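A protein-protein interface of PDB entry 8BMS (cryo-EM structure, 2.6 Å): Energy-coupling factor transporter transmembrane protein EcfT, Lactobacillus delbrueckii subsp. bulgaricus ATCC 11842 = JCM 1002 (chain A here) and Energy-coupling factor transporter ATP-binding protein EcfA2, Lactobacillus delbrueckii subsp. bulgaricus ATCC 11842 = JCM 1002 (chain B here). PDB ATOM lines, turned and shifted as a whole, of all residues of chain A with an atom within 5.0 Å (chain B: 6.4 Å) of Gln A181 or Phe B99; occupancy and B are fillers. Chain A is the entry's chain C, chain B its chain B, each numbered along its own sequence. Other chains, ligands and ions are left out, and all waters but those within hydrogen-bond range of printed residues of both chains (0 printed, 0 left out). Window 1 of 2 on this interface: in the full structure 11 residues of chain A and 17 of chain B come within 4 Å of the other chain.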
ATOM      1  N   ILE A 177       5.138   9.030  -4.678  1.00  0.00           N
ATOM      2  CA  ILE A 177       4.389  10.236  -5.033  1.00  0.00           C
ATOM      3  C   ILE A 177       4.069  11.079  -3.803  1.00  0.00           C
ATOM      4  O   ILE A 177       4.048  12.310  -3.891  1.00  0.00           O
ATOM      5  CB  ILE A 177       3.125   9.920  -5.865  1.00  0.00           C
ATOM      6  CG1 ILE A 177       3.476   9.294  -7.226  1.00  0.00           C
ATOM      7  CG2 ILE A 177       2.298  11.171  -6.105  1.00  0.00           C
ATOM      8  CD1 ILE A 177       3.599   7.810  -7.287  1.00  0.00           C
ATOM      9  N   MET A 178       3.836  10.468  -2.636  1.00  0.00           N
ATOM     10  CA  MET A 178       3.614  11.281  -1.445  1.00  0.00           C
ATOM     11  C   MET A 178       4.837  12.133  -1.123  1.00  0.00           C
ATOM     12  O   MET A 178       4.708  13.321  -0.813  1.00  0.00           O
ATOM     13  CB  MET A 178       3.241  10.396  -0.257  1.00  0.00           C
ATOM     14  CG  MET A 178       1.755  10.091  -0.163  1.00  0.00           C
ATOM     15  SD  MET A 178       1.202   9.785   1.524  1.00  0.00           S
ATOM     16  CE  MET A 178       1.946   8.188   1.839  1.00  0.00           C
ATOM     17  N   ASN A 179       6.036  11.550  -1.217  1.00  0.00           N
ATOM     18  CA  ASN A 179       7.255  12.323  -0.988  1.00  0.00           C
ATOM     19  C   ASN A 179       7.453  13.386  -2.061  1.00  0.00           C
ATOM     20  O   ASN A 179       7.844  14.520  -1.756  1.00  0.00           O
ATOM     21  CB  ASN A 179       8.463  11.390  -0.935  1.00  0.00           C
ATOM     22  CG  ASN A 179       8.614  10.709   0.408  1.00  0.00           C
ATOM     23  OD1 ASN A 179       8.271  11.273   1.446  1.00  0.00           O
ATOM     24  ND2 ASN A 179       9.131   9.486   0.395  1.00  0.00           N
ATOM     25  N   ALA A 180       7.191  13.037  -3.324  1.00  0.00           N
ATOM     26  CA  ALA A 180       7.379  13.989  -4.416  1.00  0.00           C
ATOM     27  C   ALA A 180       6.445  15.183  -4.277  1.00  0.00           C
ATOM     28  O   ALA A 180       6.833  16.321  -4.566  1.00  0.00           O
ATOM     29  CB  ALA A 180       7.166  13.294  -5.759  1.00  0.00           C
ATOM     30  N   GLN A 181       5.206  14.943  -3.849  1.00  0.00           N
ATOM     31  CA  GLN A 181       4.257  16.031  -3.653  1.00  0.00           C
ATOM     32  C   GLN A 181       4.560  16.820  -2.385  1.00  0.00           C
ATOM     33  O   GLN A 181       4.377  18.040  -2.359  1.00  0.00           O
ATOM     34  CB  GLN A 181       2.831  15.481  -3.618  1.00  0.00           C
ATOM     35  CG  GLN A 181       2.423  14.724  -4.868  1.00  0.00           C
ATOM     36  CD  GLN A 181       0.943  14.829  -5.157  1.00  0.00           C
ATOM     37  OE1 GLN A 181       0.229  15.600  -4.519  1.00  0.00           O
ATOM     38  NE2 GLN A 181       0.472  14.052  -6.123  1.00  0.00           N
ATOM     39  N   ARG A 182       5.026  16.147  -1.328  1.00  0.00           N
ATOM     40  CA  ARG A 182       5.413  16.858  -0.115  1.00  0.00           C
ATOM     41  C   ARG A 182       6.558  17.819  -0.387  1.00  0.00           C
ATOM     42  O   ARG A 182       6.538  18.964   0.074  1.00  0.00           O
ATOM     43  CB  ARG A 182       5.808  15.865   0.976  1.00  0.00           C
ATOM     44  CG  ARG A 182       4.665  15.390   1.845  1.00  0.00           C
ATOM     45  CD  ARG A 182       5.081  14.191   2.678  1.00  0.00           C
ATOM     46  NE  ARG A 182       4.024  13.771   3.589  1.00  0.00           N
ATOM     47  CZ  ARG A 182       3.684  12.509   3.809  1.00  0.00           C
ATOM     48  NH1 ARG A 182       4.302  11.510   3.200  1.00  0.00           N
ATOM     49  NH2 ARG A 182       2.698  12.242   4.661  1.00  0.00           N
ATOM     50  N   SER A 183       7.561  17.371  -1.148  1.00  0.00           N
ATOM     51  CA  SER A 183       8.719  18.213  -1.427  1.00  0.00           C
ATOM     52  C   SER A 183       8.322  19.520  -2.097  1.00  0.00           C
ATOM     53  O   SER A 183       8.963  20.553  -1.870  1.00  0.00           O
ATOM     54  CB  SER A 183       9.719  17.459  -2.300  1.00  0.00           C
ATOM     55  OG  SER A 183      10.160  16.276  -1.661  1.00  0.00           O
ATOM     56  N   ARG A 184       7.274  19.503  -2.922  1.00  0.00           N
ATOM     57  CA  ARG A 184       6.854  20.679  -3.669  1.00  0.00           C
ATOM     58  C   ARG A 184       5.621  21.353  -3.073  1.00  0.00           C
ATOM     59  O   ARG A 184       5.003  22.191  -3.735  1.00  0.00           O
ATOM     60  CB  ARG A 184       6.620  20.313  -5.134  1.00  0.00           C
ATOM     61  CG  ARG A 184       7.844  20.554  -6.006  1.00  0.00           C
ATOM     62  CD  ARG A 184       7.503  20.596  -7.483  1.00  0.00           C
ATOM     63  NE  ARG A 184       7.710  19.303  -8.120  1.00  0.00           N
ATOM     64  CZ  ARG A 184       7.041  18.874  -9.181  1.00  0.00           C
ATOM     65  NH1 ARG A 184       6.113  19.618  -9.758  1.00  0.00           N
ATOM     66  NH2 ARG A 184       7.311  17.670  -9.675  1.00  0.00           N
ATOM     67  N   GLY A 185       5.248  21.005  -1.841  1.00  0.00           N
ATOM     68  CA  GLY A 185       4.295  21.793  -1.082  1.00  0.00           C
ATOM     69  C   GLY A 185       2.957  21.154  -0.780  1.00  0.00           C
ATOM     70  O   GLY A 185       2.101  21.825  -0.194  1.00  0.00           O
ATOM     71  N   ALA A 186       2.731  19.898  -1.152  1.00  0.00           N
ATOM     72  CA  ALA A 186       1.472  19.253  -0.808  1.00  0.00           C
ATOM     73  C   ALA A 186       1.397  19.002   0.691  1.00  0.00           C
ATOM     74  O   ALA A 186       2.402  18.704   1.341  1.00  0.00           O
ATOM     75  CB  ALA A 186       1.310  17.940  -1.567  1.00  0.00           C
ATOM     76  N   PHE A 188      -0.757  16.632   3.064  1.00  0.00           N
ATOM     77  CA  PHE A 188      -1.699  15.555   3.330  1.00  0.00           C
ATOM     78  C   PHE A 188      -2.094  15.471   4.797  1.00  0.00           C
ATOM     79  O   PHE A 188      -2.916  14.622   5.156  1.00  0.00           O
ATOM     80  CB  PHE A 188      -1.114  14.212   2.881  1.00  0.00           C
ATOM     81  CG  PHE A 188      -0.526  14.238   1.501  1.00  0.00           C
ATOM     82  CD1 PHE A 188      -1.340  14.136   0.386  1.00  0.00           C
ATOM     83  CD2 PHE A 188       0.840  14.359   1.318  1.00  0.00           C
ATOM     84  CE1 PHE A 188      -0.801  14.159  -0.885  1.00  0.00           C
ATOM     85  CE2 PHE A 188       1.384  14.381   0.050  1.00  0.00           C
ATOM     86  CZ  PHE A 188       0.563  14.280  -1.052  1.00  0.00           C
ATOM     87  N   MET A 203      -4.402  11.473  -6.499  1.00  0.00           N
ATOM     88  CA  MET A 203      -3.288  10.540  -6.571  1.00  0.00           C
ATOM     89  C   MET A 203      -3.683   9.155  -7.065  1.00  0.00           C
ATOM     90  O   MET A 203      -2.797   8.379  -7.433  1.00  0.00           O
ATOM     91  CB  MET A 203      -2.637  10.399  -5.193  1.00  0.00           C
ATOM     92  CG  MET A 203      -1.946  11.645  -4.683  1.00  0.00           C
ATOM     93  SD  MET A 203      -1.297  11.385  -3.024  1.00  0.00           S
ATOM     94  CE  MET A 203       0.045  10.252  -3.366  1.00  0.00           C
ATOM     95  N   PRO A 206      -2.664   8.140 -10.868  1.00  0.00           N
ATOM     96  CA  PRO A 206      -1.205   7.977 -10.974  1.00  0.00           C
ATOM     97  C   PRO A 206      -0.677   6.755 -10.247  1.00  0.00           C
ATOM     98  O   PRO A 206       0.223   6.089 -10.766  1.00  0.00           O
ATOM     99  CB  PRO A 206      -0.666   9.277 -10.365  1.00  0.00           C
ATOM    100  CG  PRO A 206      -1.729  10.266 -10.617  1.00  0.00           C
ATOM    101  CD  PRO A 206      -3.022   9.519 -10.484  1.00  0.00           C
ATOM    102  N   GLU B  95      12.698  10.543 -12.098  1.00  0.00           N
ATOM    103  CA  GLU B  95      11.483   9.742 -12.196  1.00  0.00           C
ATOM    104  C   GLU B  95      10.697   9.775 -10.892  1.00  0.00           C
ATOM    105  O   GLU B  95       9.462   9.767 -10.904  1.00  0.00           O
ATOM    106  CB  GLU B  95      11.831   8.305 -12.582  1.00  0.00           C
ATOM    107  CG  GLU B  95      12.355   8.143 -14.005  1.00  0.00           C
ATOM    108  CD  GLU B  95      13.786   8.621 -14.169  1.00  0.00           C
ATOM    109  OE1 GLU B  95      14.527   8.640 -13.165  1.00  0.00           O
ATOM    110  OE2 GLU B  95      14.167   8.980 -15.302  1.00  0.00           O
ATOM    111  N   ALA B  96      11.396   9.818  -9.760  1.00  0.00           N
ATOM    112  CA  ALA B  96      10.769   9.893  -8.449  1.00  0.00           C
ATOM    113  C   ALA B  96      10.270  11.291  -8.108  1.00  0.00           C
ATOM    114  O   ALA B  96       9.815  11.513  -6.982  1.00  0.00           O
ATOM    115  CB  ALA B  96      11.748   9.417  -7.373  1.00  0.00           C
ATOM    116  N   GLN B  97      10.345  12.230  -9.047  1.00  0.00           N
ATOM    117  CA  GLN B  97       9.958  13.614  -8.814  1.00  0.00           C
ATOM    118  C   GLN B  97       8.788  14.079  -9.668  1.00  0.00           C
ATOM    119  O   GLN B  97       8.018  14.930  -9.219  1.00  0.00           O
ATOM    120  CB  GLN B  97      11.156  14.543  -9.064  1.00  0.00           C
ATOM    121  CG  GLN B  97      10.950  15.973  -8.605  1.00  0.00           C
ATOM    122  CD  GLN B  97      12.250  16.655  -8.238  1.00  0.00           C
ATOM    123  OE1 GLN B  97      13.312  16.312  -8.757  1.00  0.00           O
ATOM    124  NE2 GLN B  97      12.173  17.625  -7.339  1.00  0.00           N
ATOM    125  N   LEU B  98       8.626  13.542 -10.874  1.00  0.00           N
ATOM    126  CA  LEU B  98       7.587  13.976 -11.798  1.00  0.00           C
ATOM    127  C   LEU B  98       6.379  13.058 -11.678  1.00  0.00           C
ATOM    128  O   LEU B  98       6.520  11.831 -11.714  1.00  0.00           O
ATOM    129  CB  LEU B  98       8.106  13.980 -13.237  1.00  0.00           C
ATOM    130  CG  LEU B  98       9.547  14.441 -13.464  1.00  0.00           C
ATOM    131  CD1 LEU B  98       9.937  14.287 -14.923  1.00  0.00           C
ATOM    132  CD2 LEU B  98       9.748  15.874 -13.008  1.00  0.00           C
ATOM    133  N   PHE B  99       5.194  13.653 -11.530  1.00  0.00           N
ATOM    134  CA  PHE B  99       3.968  12.873 -11.405  1.00  0.00           C
ATOM    135  C   PHE B  99       2.797  13.398 -12.221  1.00  0.00           C
ATOM    136  O   PHE B  99       1.813  12.670 -12.370  1.00  0.00           O
ATOM    137  CB  PHE B  99       3.537  12.791  -9.932  1.00  0.00           C
ATOM    138  CG  PHE B  99       3.538  14.117  -9.225  1.00  0.00           C
ATOM    139  CD1 PHE B  99       2.435  14.952  -9.292  1.00  0.00           C
ATOM    140  CD2 PHE B  99       4.641  14.528  -8.498  1.00  0.00           C
ATOM    141  CE1 PHE B  99       2.436  16.170  -8.648  1.00  0.00           C
ATOM    142  CE2 PHE B  99       4.645  15.746  -7.852  1.00  0.00           C
ATOM    143  CZ  PHE B  99       3.541  16.567  -7.928  1.00  0.00           C
ATOM    144  N   GLU B 100       2.855  14.615 -12.750  1.00  0.00           N
ATOM    145  CA  GLU B 100       1.695  15.232 -13.372  1.00  0.00           C
ATOM    146  C   GLU B 100       1.572  14.799 -14.834  1.00  0.00           C
ATOM    147  O   GLU B 100       2.472  14.185 -15.409  1.00  0.00           O
ATOM    148  CB  GLU B 100       1.786  16.753 -13.254  1.00  0.00           C
ATOM    149  CG  GLU B 100       0.460  17.477 -13.387  1.00  0.00           C
ATOM    150  CD  GLU B 100      -0.395  17.369 -12.143  1.00  0.00           C
ATOM    151  OE1 GLU B 100       0.176  17.269 -11.037  1.00  0.00           O
ATOM    152  OE2 GLU B 100      -1.637  17.388 -12.269  1.00  0.00           O
ATOM    153  N   ASN B 101       0.423  15.126 -15.435  1.00  0.00           N
ATOM    154  CA  ASN B 101       0.120  14.655 -16.784  1.00  0.00           C
ATOM    155  C   ASN B 101       1.045  15.267 -17.829  1.00  0.00           C
ATOM    156  O   ASN B 101       1.529  14.561 -18.720  1.00  0.00           O
ATOM    157  CB  ASN B 101      -1.338  14.951 -17.129  1.00  0.00           C
ATOM    158  CG  ASN B 101      -2.309  14.209 -16.236  1.00  0.00           C
ATOM    159  OD1 ASN B 101      -2.463  12.993 -16.343  1.00  0.00           O
ATOM    160  ND2 ASN B 101      -2.975  14.940 -15.350  1.00  0.00           N
ATOM    161  N   ASP B 106       3.211  19.914 -14.485  1.00  0.00           N
ATOM    162  CA  ASP B 106       4.178  19.443 -13.499  1.00  0.00           C
ATOM    163  C   ASP B 106       5.068  20.571 -12.994  1.00  0.00           C
ATOM    164  O   ASP B 106       5.324  20.677 -11.789  1.00  0.00           O
ATOM    165  CB  ASP B 106       5.025  18.330 -14.111  1.00  0.00           C
ATOM    166  CG  ASP B 106       5.671  17.449 -13.072  1.00  0.00           C
ATOM    167  OD1 ASP B 106       4.972  17.024 -12.127  1.00  0.00           O
ATOM    168  OD2 ASP B 106       6.880  17.183 -13.203  1.00  0.00           O
ATOM    169  N   TYR B 109       3.078  22.944 -10.811  1.00  0.00           N
ATOM    170  CA  TYR B 109       2.534  22.372  -9.584  1.00  0.00           C
ATOM    171  C   TYR B 109       3.082  23.080  -8.349  1.00  0.00           C
ATOM    172  O   TYR B 109       2.331  23.409  -7.424  1.00  0.00           O
ATOM    173  CB  TYR B 109       2.853  20.877  -9.529  1.00  0.00           C
ATOM    174  CG  TYR B 109       2.374  20.197  -8.271  1.00  0.00           C
ATOM    175  CD1 TYR B 109       1.053  19.803  -8.136  1.00  0.00           C
ATOM    176  CD2 TYR B 109       3.242  19.950  -7.217  1.00  0.00           C
ATOM    177  CE1 TYR B 109       0.608  19.182  -6.990  1.00  0.00           C
ATOM    178  CE2 TYR B 109       2.807  19.331  -6.065  1.00  0.00           C
ATOM    179  CZ  TYR B 109       1.488  18.949  -5.957  1.00  0.00           C
ATOM    180  OH  TYR B 109       1.046  18.330  -4.814  1.00  0.00           O
ATOM    181  N   ASN B 113       0.991  25.544  -5.257  1.00  0.00           N
ATOM    182  CA  ASN B 113       0.896  25.250  -3.836  1.00  0.00           C
ATOM    183  C   ASN B 113       1.345  26.418  -2.976  1.00  0.00           C
ATOM    184  O   ASN B 113       0.958  26.489  -1.807  1.00  0.00           O
ATOM    185  CB  ASN B 113       1.734  24.016  -3.495  1.00  0.00           C
ATOM    186  CG  ASN B 113       1.091  22.728  -3.961  1.00  0.00           C
ATOM    187  OD1 ASN B 113      -0.095  22.693  -4.280  1.00  0.00           O
ATOM    188  ND2 ASN B 113       1.870  21.655  -3.983  1.00  0.00           N
ATOM    189  N   PRO B 143       5.626  14.111 -18.876  1.00  0.00           N
ATOM    190  CA  PRO B 143       7.003  14.091 -18.362  1.00  0.00           C
ATOM    191  C   PRO B 143       7.679  12.741 -18.501  1.00  0.00           C
ATOM    192  O   PRO B 143       8.914  12.675 -18.462  1.00  0.00           O
ATOM    193  CB  PRO B 143       6.836  14.485 -16.887  1.00  0.00           C
ATOM    194  CG  PRO B 143       5.487  15.110 -16.793  1.00  0.00           C
ATOM    195  CD  PRO B 143       4.648  14.443 -17.830  1.00  0.00           C
ATOM    196  N   PHE B 144       6.913  11.665 -18.658  1.00  0.00           N
ATOM    197  CA  PHE B 144       7.467  10.326 -18.795  1.00  0.00           C
ATOM    198  C   PHE B 144       7.720   9.929 -20.242  1.00  0.00           C
ATOM    199  O   PHE B 144       8.429   8.948 -20.482  1.00  0.00           O
ATOM    200  CB  PHE B 144       6.531   9.312 -18.131  1.00  0.00           C
ATOM    201  CG  PHE B 144       5.924   9.809 -16.853  1.00  0.00           C
ATOM    202  CD1 PHE B 144       6.671   9.850 -15.688  1.00  0.00           C
ATOM    203  CD2 PHE B 144       4.613  10.252 -16.820  1.00  0.00           C
ATOM    204  CE1 PHE B 144       6.117  10.314 -14.512  1.00  0.00           C
ATOM    205  CE2 PHE B 144       4.055  10.718 -15.645  1.00  0.00           C
ATOM    206  CZ  PHE B 144       4.808  10.748 -14.491  1.00  0.00           C
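OD1 of Asp B106 lies within hydrogen-bond range of N of Glu B100 (3.3 Å). The backbone NH of Ala A186 lies within hydrogen-bond range of the backbone carbonyl oxygen of Gln A181. OD1 of Asp B106 lies within hydrogen-bond range of N of Phe B99.
Ala A180 touches Ala B96 (CB to O, 3.4 Å). CB of Ala A180 touches O of Gln B97 (3.9 Å). CB of Ala A180 touches CD2 of Phe B99, 3.9 Å away. CZ of Phe B99 touches CG of Gln A181, at 3.7 Å. NH2 of Arg A184 touches CE2 of Phe B99, at 3.8 Å. Arg A184 touches Tyr B109. Gly A185 touches Asn B113. Tyr B109 touches Ala A186.
Of the 13 printed residues of chain A, 5 touch a printed residue of chain B. Of the 12 printed residues of chain B, 6 touch a printed residue of chain A. Printed residues of chain B that touch a printed residue of chain A: Ala B96, Gln B97, Phe B99, Asp B106, Tyr B109 and Asn B113. Hydrophobic or aromatic side chains of chain B within 4 Å of the printed part of chain A: Phe B99 and Tyr B109. Among the printed residues, Asp or Glu carboxylates within 4 Å of a Lys or Arg side-chain nitrogen of the other chain: Arg A184 with Asp B106 (3.4 Å).
NH2 of Arg A184 is in salt-bridge range of OD1 of Asp B106. The backbone NH of Ala A186 sits close to the side-chain amide nitrogen of Asn B113 (3.4 Å). ND2 of Asn B113 is in hydrogen-bond range of O of Arg A184. OE1 of Gln A181 is in hydrogen-bond range of OH of Tyr B109 (2.9 Å). The backbone carbonyl oxygen (O) of Gln B97 sits at hydrogen-bond distance from the guanidinium group (NH2) of Arg A184 (2.9 Å).
Of chain A, only Ala A180, Gln A181 and Arg A184 come within 4 Å of Phe B99. Of the printed residues of chain B, Gly A185 touches Asn B113 (3.4 Å). Printed residues of chain B within 4 Å of Ala A180: Ala B96, Gln B97 and Phe B99. Printed residues of chain A within 4 Å of Asp B106: Arg A184 (2.4 Å). Of the printed residues of chain A, Asn B113 touches Arg A184 (3.2 Å), Gly A185 (3.4 Å) and Ala A186 (3.4 Å). Ile A177 touches none of the printed residues of chain B. Met A178 touches none of the printed residues of chain B. The nearest residue of chain A that does not touch Phe B99 is Ile A177 (4.3 Å). The nearest printed residue of chain B that does not touch Ala A186 is Phe B99 (6.9 Å).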
